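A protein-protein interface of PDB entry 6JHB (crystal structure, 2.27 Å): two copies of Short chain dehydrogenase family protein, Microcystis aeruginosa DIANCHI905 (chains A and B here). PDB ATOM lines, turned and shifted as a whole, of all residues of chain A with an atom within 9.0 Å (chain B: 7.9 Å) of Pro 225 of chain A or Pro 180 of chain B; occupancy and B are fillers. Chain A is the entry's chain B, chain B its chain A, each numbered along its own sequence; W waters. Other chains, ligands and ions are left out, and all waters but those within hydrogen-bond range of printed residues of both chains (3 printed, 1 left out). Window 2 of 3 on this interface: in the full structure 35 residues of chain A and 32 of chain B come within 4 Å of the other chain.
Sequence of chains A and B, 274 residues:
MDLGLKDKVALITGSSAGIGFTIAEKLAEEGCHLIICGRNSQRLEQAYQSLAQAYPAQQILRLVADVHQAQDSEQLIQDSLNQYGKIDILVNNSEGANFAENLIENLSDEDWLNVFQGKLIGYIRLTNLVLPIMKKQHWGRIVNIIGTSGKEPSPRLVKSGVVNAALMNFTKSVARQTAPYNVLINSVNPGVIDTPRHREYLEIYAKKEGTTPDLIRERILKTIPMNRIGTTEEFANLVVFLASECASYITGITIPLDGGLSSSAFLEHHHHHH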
ATOM      1  N   ILE A 220      22.495 -20.091  25.638  1.00  0.00           N
ATOM      2  CA  ILE A 220      22.279 -18.724  25.158  1.00  0.00           C
ATOM      3  C   ILE A 220      23.331 -18.381  24.107  1.00  0.00           C
ATOM      4  O   ILE A 220      22.984 -17.979  23.002  1.00  0.00           O
ATOM      5  CB  ILE A 220      22.372 -17.688  26.298  1.00  0.00           C
ATOM      6  CG1 ILE A 220      21.339 -18.017  27.386  1.00  0.00           C
ATOM      7  CG2 ILE A 220      22.230 -16.282  25.731  1.00  0.00           C
ATOM      8  CD1 ILE A 220      20.799 -16.837  28.163  1.00  0.00           C
ATOM      9  N   LEU A 221      24.595 -18.571  24.481  1.00  0.00           N
ATOM     10  CA  LEU A 221      25.754 -18.302  23.631  1.00  0.00           C
ATOM     11  C   LEU A 221      25.719 -18.958  22.248  1.00  0.00           C
ATOM     12  O   LEU A 221      26.149 -18.356  21.259  1.00  0.00           O
ATOM     13  CB  LEU A 221      27.027 -18.741  24.349  1.00  0.00           C
ATOM     14  CG  LEU A 221      27.407 -17.848  25.532  1.00  0.00           C
ATOM     15  CD1 LEU A 221      28.523 -18.480  26.349  1.00  0.00           C
ATOM     16  CD2 LEU A 221      27.813 -16.467  25.049  1.00  0.00           C
ATOM     17  N   LYS A 222      25.202 -20.177  22.184  1.00  0.00           N
ATOM     18  CA  LYS A 222      25.107 -20.896  20.926  1.00  0.00           C
ATOM     19  C   LYS A 222      24.138 -20.173  20.002  1.00  0.00           C
ATOM     20  O   LYS A 222      24.248 -20.260  18.775  1.00  0.00           O
ATOM     21  CB  LYS A 222      24.633 -22.335  21.159  1.00  0.00           C
ATOM     22  N   THR A 223      23.190 -19.445  20.583  1.00  0.00           N
ATOM     23  CA  THR A 223      22.225 -18.692  19.778  1.00  0.00           C
ATOM     24  C   THR A 223      22.670 -17.272  19.418  1.00  0.00           C
ATOM     25  O   THR A 223      22.020 -16.628  18.590  1.00  0.00           O
ATOM     26  CB  THR A 223      20.868 -18.574  20.482  1.00  0.00           C
ATOM     27  OG1 THR A 223      21.013 -17.755  21.649  1.00  0.00           O
ATOM     28  CG2 THR A 223      20.337 -19.962  20.869  1.00  0.00           C
ATOM     29  N   ILE A 224      23.729 -16.766  20.045  1.00  0.00           N
ATOM     30  CA  ILE A 224      24.236 -15.424  19.716  1.00  0.00           C
ATOM     31  C   ILE A 224      25.310 -15.580  18.663  1.00  0.00           C
ATOM     32  O   ILE A 224      26.291 -16.288  18.891  1.00  0.00           O
ATOM     33  CB  ILE A 224      24.845 -14.698  20.924  1.00  0.00           C
ATOM     34  CG1 ILE A 224      23.762 -14.388  21.979  1.00  0.00           C
ATOM     35  CG2 ILE A 224      25.505 -13.390  20.489  1.00  0.00           C
ATOM     36  CD1 ILE A 224      24.323 -14.095  23.359  1.00  0.00           C
ATOM     37  N   PRO A 225      25.143 -14.931  17.504  1.00  0.00           N
ATOM     38  CA  PRO A 225      26.142 -15.166  16.464  1.00  0.00           C
ATOM     39  C   PRO A 225      27.557 -14.747  16.847  1.00  0.00           C
ATOM     40  O   PRO A 225      28.514 -15.437  16.493  1.00  0.00           O
ATOM     41  CB  PRO A 225      25.601 -14.376  15.279  1.00  0.00           C
ATOM     42  CG  PRO A 225      24.132 -14.415  15.478  1.00  0.00           C
ATOM     43  CD  PRO A 225      23.908 -14.352  16.953  1.00  0.00           C
ATOM     44  N   MET A 226      27.714 -13.668  17.601  1.00  0.00           N
ATOM     45  CA  MET A 226      29.041 -13.366  18.130  1.00  0.00           C
ATOM     46  C   MET A 226      29.532 -14.358  19.181  1.00  0.00           C
ATOM     47  O   MET A 226      30.678 -14.278  19.593  1.00  0.00           O
ATOM     48  CB  MET A 226      29.108 -11.963  18.689  1.00  0.00           C
ATOM     49  CG  MET A 226      29.128 -10.913  17.599  1.00  0.00           C
ATOM     50  SD  MET A 226      29.320  -9.248  18.233  1.00  0.00           S
ATOM     51  CE  MET A 226      30.855  -9.483  19.078  1.00  0.00           C
ATOM     52  N   ASN A 227      28.694 -15.297  19.611  1.00  0.00           N
ATOM     53  CA  ASN A 227      29.134 -16.316  20.565  1.00  0.00           C
ATOM     54  C   ASN A 227      29.660 -15.694  21.866  1.00  0.00           C
ATOM     55  O   ASN A 227      30.598 -16.202  22.456  1.00  0.00           O
ATOM     56  CB  ASN A 227      30.206 -17.227  19.937  1.00  0.00           C
ATOM     57  CG  ASN A 227      30.390 -18.537  20.696  1.00  0.00           C
ATOM     58  N   ARG A 228      29.080 -14.574  22.293  1.00  0.00           N
ATOM     59  CA  ARG A 228      29.406 -14.012  23.598  1.00  0.00           C
ATOM     60  C   ARG A 228      28.307 -13.092  24.076  1.00  0.00           C
ATOM     61  O   ARG A 228      27.488 -12.596  23.306  1.00  0.00           O
ATOM     62  CB  ARG A 228      30.776 -13.333  23.611  1.00  0.00           C
ATOM     63  CG  ARG A 228      30.818 -11.939  23.071  1.00  0.00           C
ATOM     64  CD  ARG A 228      32.219 -11.351  23.195  1.00  0.00           C
ATOM     65  NE  ARG A 228      32.261 -10.204  22.331  1.00  0.00           N
ATOM     66  CZ  ARG A 228      31.734  -9.025  22.620  1.00  0.00           C
ATOM     67  NH1 ARG A 228      31.174  -8.791  23.812  1.00  0.00           N
ATOM     68  NH2 ARG A 228      31.794  -8.059  21.713  1.00  0.00           N
ATOM     69  N   ILE A 229      28.281 -12.902  25.373  1.00  0.00           N
ATOM     70  CA  ILE A 229      27.291 -12.075  26.024  1.00  0.00           C
ATOM     71  C   ILE A 229      27.850 -10.660  26.063  1.00  0.00           C
ATOM     72  O   ILE A 229      29.010 -10.475  26.354  1.00  0.00           O
ATOM     73  CB  ILE A 229      27.057 -12.602  27.454  1.00  0.00           C
ATOM     74  CG1 ILE A 229      26.636 -14.076  27.352  1.00  0.00           C
ATOM     75  CG2 ILE A 229      26.082 -11.710  28.211  1.00  0.00           C
ATOM     76  CD1 ILE A 229      25.371 -14.486  28.069  1.00  0.00           C
ATOM     77  N   ASP A 258      22.655  -6.549  20.281  1.00  0.00           N
ATOM     78  CA  ASP A 258      22.414  -7.948  20.656  1.00  0.00           C
ATOM     79  C   ASP A 258      23.374  -9.013  20.113  1.00  0.00           C
ATOM     80  O   ASP A 258      23.032 -10.190  20.095  1.00  0.00           O
ATOM     81  CB  ASP A 258      21.038  -8.300  20.163  1.00  0.00           C
ATOM     82  CG  ASP A 258      20.934  -8.190  18.646  1.00  0.00           C
ATOM     83  OD1 ASP A 258      19.820  -8.227  18.121  1.00  0.00           O
ATOM     84  OD2 ASP A 258      21.970  -8.070  17.963  1.00  0.00           O
ATOM     85  N   GLY A 259      24.555  -8.613  19.675  1.00  0.00           N
ATOM     86  CA  GLY A 259      25.518  -9.548  19.096  1.00  0.00           C
ATOM     87  C   GLY A 259      25.002 -10.399  17.942  1.00  0.00           C
ATOM     88  O   GLY A 259      25.528 -11.482  17.700  1.00  0.00           O
ATOM     89  N   GLY A 260      23.977  -9.921  17.237  1.00  0.00           N
ATOM     90  CA  GLY A 260      23.447 -10.603  16.051  1.00  0.00           C
ATOM     91  C   GLY A 260      22.223 -11.450  16.305  1.00  0.00           C
ATOM     92  O   GLY A 260      21.672 -12.044  15.379  1.00  0.00           O
ATOM     93  N   LEU A 261      21.784 -11.480  17.561  1.00  0.00           N
ATOM     94  CA  LEU A 261      20.638 -12.276  17.980  1.00  0.00           C
ATOM     95  C   LEU A 261      19.435 -12.108  17.035  1.00  0.00           C
ATOM     96  O   LEU A 261      18.795 -13.086  16.655  1.00  0.00           O
ATOM     97  CB  LEU A 261      20.261 -11.905  19.413  1.00  0.00           C
ATOM     98  CG  LEU A 261      19.715 -12.981  20.342  1.00  0.00           C
ATOM     99  CD1 LEU A 261      20.651 -14.168  20.399  1.00  0.00           C
ATOM    100  CD2 LEU A 261      19.500 -12.408  21.739  1.00  0.00           C
ATOM    101  N   SER A 262      19.158 -10.874  16.634  1.00  0.00           N
ATOM    102  CA  SER A 262      18.088 -10.591  15.663  1.00  0.00           C
ATOM    103  C   SER A 262      18.343 -11.151  14.253  1.00  0.00           C
ATOM    104  O   SER A 262      17.403 -11.467  13.531  1.00  0.00           O
ATOM    105  CB  SER A 262      17.850  -9.081  15.557  1.00  0.00           C
ATOM    106  OG  SER A 262      18.759  -8.471  14.648  1.00  0.00           O
ATOM    107  N   SER A 263      19.601 -11.268  13.847  1.00  0.00           N
ATOM    108  CA  SER A 263      19.894 -11.822  12.528  1.00  0.00           C
ATOM    109  C   SER A 263      19.828 -13.363  12.502  1.00  0.00           C
ATOM    110  O   SER A 263      19.926 -13.971  11.439  1.00  0.00           O
ATOM    111  CB  SER A 263      21.246 -11.329  12.014  1.00  0.00           C
ATOM    112  OG  SER A 263      22.293 -12.192  12.420  1.00  0.00           O
ATOM    113  N   SER A 264      19.661 -13.978  13.670  1.00  0.00           N
ATOM    114  CA  SER A 264      19.489 -15.425  13.786  1.00  0.00           C
ATOM    115  C   SER A 264      18.024 -15.783  14.064  1.00  0.00           C
ATOM    116  O   SER A 264      17.234 -16.016  13.142  1.00  0.00           O
ATOM    117  CB  SER A 264      20.362 -15.956  14.919  1.00  0.00           C
ATOM    118  OG  SER A 264      19.806 -15.604  16.181  1.00  0.00           O
ATOM    119  N   LYS B 135      38.355 -11.212   8.130  1.00  0.00           N
ATOM    120  CA  LYS B 135      38.411 -12.457   8.940  1.00  0.00           C
ATOM    121  C   LYS B 135      39.834 -12.799   9.388  1.00  0.00           C
ATOM    122  O   LYS B 135      40.064 -13.216  10.529  1.00  0.00           O
ATOM    123  CB  LYS B 135      37.818 -13.645   8.182  1.00  0.00           C
ATOM    124  CG  LYS B 135      36.313 -13.531   8.014  1.00  0.00           C
ATOM    125  CD  LYS B 135      35.762 -14.337   6.847  1.00  0.00           C
ATOM    126  CE  LYS B 135      35.533 -15.789   7.204  1.00  0.00           C
ATOM    127  NZ  LYS B 135      34.434 -16.374   6.377  1.00  0.00           N
ATOM    128  N   HIS B 138      40.619 -10.628  12.105  1.00  0.00           N
ATOM    129  CA  HIS B 138      39.684 -10.724  13.205  1.00  0.00           C
ATOM    130  C   HIS B 138      39.131  -9.366  13.576  1.00  0.00           C
ATOM    131  O   HIS B 138      38.808  -9.107  14.708  1.00  0.00           O
ATOM    132  CB  HIS B 138      40.350 -11.361  14.413  1.00  0.00           C
ATOM    133  CG  HIS B 138      40.200 -12.831  14.435  1.00  0.00           C
ATOM    134  ND1 HIS B 138      40.984 -13.664  13.669  1.00  0.00           N
ATOM    135  CD2 HIS B 138      39.324 -13.623  15.089  1.00  0.00           C
ATOM    136  CE1 HIS B 138      40.611 -14.914  13.871  1.00  0.00           C
ATOM    137  NE2 HIS B 138      39.606 -14.917  14.731  1.00  0.00           N
ATOM    138  N   LYS B 172      21.816  -9.094   7.008  1.00  0.00           N
ATOM    139  CA  LYS B 172      21.454 -10.040   8.058  1.00  0.00           C
ATOM    140  C   LYS B 172      22.220 -11.350   7.967  1.00  0.00           C
ATOM    141  O   LYS B 172      22.815 -11.811   8.951  1.00  0.00           O
ATOM    142  CB  LYS B 172      19.944 -10.355   8.015  1.00  0.00           C
ATOM    143  CG  LYS B 172      19.094  -9.484   8.921  1.00  0.00           C
ATOM    144  CD  LYS B 172      17.603  -9.790   8.767  1.00  0.00           C
ATOM    145  N   VAL B 174      24.903 -12.214   6.115  1.00  0.00           N
ATOM    146  CA  VAL B 174      26.347 -12.141   6.167  1.00  0.00           C
ATOM    147  C   VAL B 174      26.828 -11.808   7.578  1.00  0.00           C
ATOM    148  O   VAL B 174      27.805 -12.399   8.033  1.00  0.00           O
ATOM    149  CB  VAL B 174      26.963 -11.225   5.085  1.00  0.00           C
ATOM    150  CG1 VAL B 174      26.678  -9.756   5.335  1.00  0.00           C
ATOM    151  CG2 VAL B 174      28.463 -11.462   5.009  1.00  0.00           C
ATOM    152  N   ALA B 175      26.124 -10.927   8.291  1.00  0.00           N
ATOM    153  CA  ALA B 175      26.458 -10.660   9.701  1.00  0.00           C
ATOM    154  C   ALA B 175      26.488 -11.932  10.561  1.00  0.00           C
ATOM    155  O   ALA B 175      27.449 -12.192  11.307  1.00  0.00           O
ATOM    156  CB  ALA B 175      25.469  -9.689  10.288  1.00  0.00           C
ATOM    157  N   ARG B 176      25.421 -12.716  10.445  1.00  0.00           N
ATOM    158  CA  ARG B 176      25.295 -14.000  11.136  1.00  0.00           C
ATOM    159  C   ARG B 176      26.551 -14.868  10.945  1.00  0.00           C
ATOM    160  O   ARG B 176      27.145 -15.354  11.890  1.00  0.00           O
ATOM    161  CB  ARG B 176      24.046 -14.722  10.628  1.00  0.00           C
ATOM    162  CG  ARG B 176      23.629 -15.931  11.454  1.00  0.00           C
ATOM    163  N   GLN B 177      26.995 -14.974   9.710  1.00  0.00           N
ATOM    164  CA  GLN B 177      28.138 -15.782   9.368  1.00  0.00           C
ATOM    165  C   GLN B 177      29.496 -15.269   9.821  1.00  0.00           C
ATOM    166  O   GLN B 177      30.373 -16.048  10.099  1.00  0.00           O
ATOM    167  CB  GLN B 177      28.183 -15.969   7.847  1.00  0.00           C
ATOM    168  CG  GLN B 177      27.739 -17.342   7.421  1.00  0.00           C
ATOM    169  CD  GLN B 177      27.727 -17.501   5.916  1.00  0.00           C
ATOM    170  OE1 GLN B 177      28.735 -17.248   5.243  1.00  0.00           O
ATOM    171  NE2 GLN B 177      26.576 -17.904   5.373  1.00  0.00           N
ATOM    172  N   THR B 178      29.712 -13.967   9.830  1.00  0.00           N
ATOM    173  CA  THR B 178      31.046 -13.461  10.107  1.00  0.00           C
ATOM    174  C   THR B 178      31.198 -12.862  11.494  1.00  0.00           C
ATOM    175  O   THR B 178      32.288 -12.379  11.844  1.00  0.00           O
ATOM    176  CB  THR B 178      31.401 -12.344   9.146  1.00  0.00           C
ATOM    177  OG1 THR B 178      30.508 -11.245   9.367  1.00  0.00           O
ATOM    178  CG2 THR B 178      31.263 -12.805   7.738  1.00  0.00           C
ATOM    179  N   ALA B 179      30.114 -12.870  12.269  1.00  0.00           N
ATOM    180  CA  ALA B 179      30.128 -12.373  13.629  1.00  0.00           C
ATOM    181  C   ALA B 179      31.165 -13.124  14.435  1.00  0.00           C
ATOM    182  O   ALA B 179      31.871 -12.506  15.203  1.00  0.00           O
ATOM    183  CB  ALA B 179      28.748 -12.495  14.274  1.00  0.00           C
ATOM    184  N   PRO B 180      31.296 -14.450  14.223  1.00  0.00           N
ATOM    185  CA  PRO B 180      32.331 -15.191  14.943  1.00  0.00           C
ATOM    186  C   PRO B 180      33.765 -14.687  14.750  1.00  0.00           C
ATOM    187  O   PRO B 180      34.652 -15.088  15.515  1.00  0.00           O
ATOM    188  CB  PRO B 180      32.203 -16.612  14.381  1.00  0.00           C
ATOM    189  CG  PRO B 180      30.790 -16.722  13.965  1.00  0.00           C
ATOM    190  CD  PRO B 180      30.371 -15.351  13.520  1.00  0.00           C
ATOM    191  N   TYR B 181      33.982 -13.821  13.760  1.00  0.00           N
ATOM    192  CA  TYR B 181      35.328 -13.296  13.428  1.00  0.00           C
ATOM    193  C   TYR B 181      35.462 -11.823  13.755  1.00  0.00           C
ATOM    194  O   TYR B 181      36.390 -11.162  13.286  1.00  0.00           O
ATOM    195  CB  TYR B 181      35.617 -13.491  11.937  1.00  0.00           C
ATOM    196  CG  TYR B 181      35.570 -14.936  11.542  1.00  0.00           C
ATOM    197  CD1 TYR B 181      36.726 -15.706  11.537  1.00  0.00           C
ATOM    198  CD2 TYR B 181      34.361 -15.551  11.225  1.00  0.00           C
ATOM    199  CE1 TYR B 181      36.689 -17.050  11.205  1.00  0.00           C
ATOM    200  CE2 TYR B 181      34.307 -16.895  10.891  1.00  0.00           C
ATOM    201  CZ  TYR B 181      35.471 -17.635  10.880  1.00  0.00           C
ATOM    202  OH  TYR B 181      35.429 -18.959  10.551  1.00  0.00           O
ATOM    203  N   ASN B 182      34.519 -11.306  14.541  1.00  0.00           N
ATOM    204  CA  ASN B 182      34.478  -9.893  14.848  1.00  0.00           C
ATOM    205  C   ASN B 182      34.521  -9.067  13.559  1.00  0.00           C
ATOM    206  O   ASN B 182      35.223  -8.059  13.483  1.00  0.00           O
ATOM    207  CB  ASN B 182      35.638  -9.519  15.783  1.00  0.00           C
ATOM    208  CG  ASN B 182      35.684  -8.022  16.107  1.00  0.00           C
ATOM    209  OD1 ASN B 182      34.635  -7.379  16.321  1.00  0.00           O
ATOM    210  ND2 ASN B 182      36.894  -7.455  16.128  1.00  0.00           N
ATOM    211  N   VAL B 183      33.813  -9.536  12.537  1.00  0.00           N
ATOM    212  CA  VAL B 183      33.573  -8.743  11.360  1.00  0.00           C
ATOM    213  C   VAL B 183      32.082  -8.426  11.350  1.00  0.00           C
ATOM    214  O   VAL B 183      31.250  -9.280  11.077  1.00  0.00           O
ATOM    215  CB  VAL B 183      34.026  -9.477  10.091  1.00  0.00           C
ATOM    216  CG1 VAL B 183      33.601  -8.708   8.855  1.00  0.00           C
ATOM    217  CG2 VAL B 183      35.539  -9.661  10.135  1.00  0.00           C
ATOM    218  N   LEU B 184      31.762  -7.191  11.689  1.00  0.00           N
ATOM    219  CA  LEU B 184      30.390  -6.781  11.930  1.00  0.00           C
ATOM    220  C   LEU B 184      29.900  -6.114  10.696  1.00  0.00           C
ATOM    221  O   LEU B 184      30.633  -5.388  10.030  1.00  0.00           O
ATOM    222  CB  LEU B 184      30.314  -5.817  13.110  1.00  0.00           C
ATOM    223  CG  LEU B 184      31.158  -6.314  14.279  1.00  0.00           C
ATOM    224  CD1 LEU B 184      30.985  -5.430  15.502  1.00  0.00           C
ATOM    225  CD2 LEU B 184      30.810  -7.768  14.608  1.00  0.00           C
ATOM    226  N   TYR B 249      29.261  -4.786  19.680  1.00  0.00           N
ATOM    227  CA  TYR B 249      28.211  -5.746  19.971  1.00  0.00           C
ATOM    228  C   TYR B 249      27.025  -5.583  19.053  1.00  0.00           C
ATOM    229  O   TYR B 249      25.999  -6.224  19.249  1.00  0.00           O
ATOM    230  CB  TYR B 249      27.743  -5.621  21.427  1.00  0.00           C
ATOM    231  CG  TYR B 249      27.169  -6.907  21.918  1.00  0.00           C
ATOM    232  CD1 TYR B 249      25.827  -7.020  22.289  1.00  0.00           C
ATOM    233  CD2 TYR B 249      27.956  -8.028  21.963  1.00  0.00           C
ATOM    234  CE1 TYR B 249      25.308  -8.235  22.730  1.00  0.00           C
ATOM    235  CE2 TYR B 249      27.458  -9.236  22.380  1.00  0.00           C
ATOM    236  CZ  TYR B 249      26.141  -9.342  22.777  1.00  0.00           C
ATOM    237  OH  TYR B 249      25.718 -10.589  23.172  1.00  0.00           O
ATOM    238  N   THR B 251      25.591  -5.952  15.326  1.00  0.00           N
ATOM    239  CA  THR B 251      25.713  -6.411  13.985  1.00  0.00           C
ATOM    240  C   THR B 251      24.392  -6.938  13.446  1.00  0.00           C
ATOM    241  O   THR B 251      23.514  -7.352  14.212  1.00  0.00           O
ATOM    242  CB  THR B 251      26.853  -7.434  13.892  1.00  0.00           C
ATOM    243  OG1 THR B 251      27.206  -7.616  12.517  1.00  0.00           O
ATOM    244  CG2 THR B 251      26.462  -8.773  14.563  1.00  0.00           C
HETATM  245  O   HOH W   1      22.796 -10.635  22.607  1.00  0.00           O
HETATM  246  O   HOH W   2      21.060  -8.503  15.352  1.00  0.00           O
HETATM  247  O   HOH W   3      22.978  -5.635  17.140  1.00  0.00           O
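Water W2 lies within hydrogen-bond range of OG of Ser 262 of chain A, OD2 of Asp 258 of chain A, O of Thr 251 of chain B and N of Ser 263 of chain A.
Water W1 bridges O of Asp 258 of chain A (2.6 Å) and OH of Tyr 249 of chain B (3.0 Å).
Water W3 lies within hydrogen-bond range of OD2 of Asp 258 of chain A (2.8 Å) and N of Thr 251 of chain B (3.2 Å).
No position is printed for both chains.
The backbone NH (N) of Gly 259 of chain A is in hydrogen-bond range of the backbone carbonyl oxygen (O) of Tyr 249 of chain B (2.8 Å).
OH of Tyr 249 of chain B is in hydrogen-bond range of O of Arg 228 of chain A, at 2.7 Å.
Tyr 249 of chain B touches Ile 224 of chain A (OH to CD1, 3.8 Å).
CB of Pro 225 of chain A touches O of Arg 176 of chain B (3.9 Å).
Pro 225 of chain A touches Ala 179 of chain B (C to CB, 3.6 Å).
CD of Pro 180 of chain B touches O of Pro 225 of chain A, 3.5 Å away.
Ala 179 of chain B touches Met 226 of chain A (CB to N, 3.7 Å).
Ile 229 of chain A touches Tyr 249 of chain B.
CE1 of Tyr 249 of chain B touches C of Asp 258 of chain A, 3.3 Å away.
Gly 260 of chain A touches Thr 251 of chain B.
Ser 263 of chain A touches Lys 172 of chain B.
OG of Ser 263 of chain A touches CB of Arg 176 of chain B (3.6 Å).
Printed residues of chain B that touch a printed residue of chain A: Lys 172, Arg 176, Ala 179, Pro 180, Tyr 249 and Thr 251.
Hydrophobic or aromatic side chains of chain B that line the printed part of chain A: Ala 179, Pro 180 and Tyr 249.
Printed residues of chain A that touch a printed residue of chain B: Ile 224, Pro 225, Met 226, Arg 228, Ile 229, Asp 258, Gly 259, Gly 260 and Ser 263.
Among the printed residues, 12 pairs touch across the chains.
Of chain B, only Arg 176 (3.9 Å), Ala 179 (3.6 Å) and Pro 180 (3.5 Å) come within 4 Å of Pro 225 of chain A.
Printed residues of chain B within 4 Å of Arg 228 of chain A: Tyr 249.
Of the printed residues of chain B, Gly 260 of chain A touches Thr 251.
Ala 179 of chain B touches just these residues of chain A: Pro 225 and Met 226.
Of the printed residues of chain A, Pro 180 of chain B touches Pro 225.
Of the printed residues of chain A, Tyr 249 of chain B touches Ile 224, Arg 228, Ile 229, Asp 258 and Gly 259.
The nearest residue of chain B that does not touch Pro 225 of chain A is Ala 175 of chain B (4.9 Å).
The nearest residue of chain A that does not touch Pro 180 of chain B is Met 226 of chain A (4.6 Å).
The nearest printed residue of chain A that does not touch Arg 176 of chain B is Ser 264 of chain A (4.8 Å).
OD1 of Asp 258 of chain A sits at hydrogen-bond distance from N of Ser 262 of chain A (3.1 Å).
The backbone carbonyl oxygen (O) of Gly 259 of chain A is in hydrogen-bond range of the backbone NH (N) of Met 226 of chain A (3.1 Å).
The side-chain carboxylate (OD2) of Asp 258 of chain A lies within hydrogen-bond range of the backbone NH (N) of Leu 261 of chain A, at 3.4 Å.
OD2 of Asp 258 of chain A lies within hydrogen-bond range of N of Gly 260 of chain A (2.8 Å).
The backbone carbonyl oxygen (O) of Gly 260 of chain A sits at hydrogen-bond distance from the side-chain hydroxyl (OG) of Ser 263 of chain A (3.0 Å).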
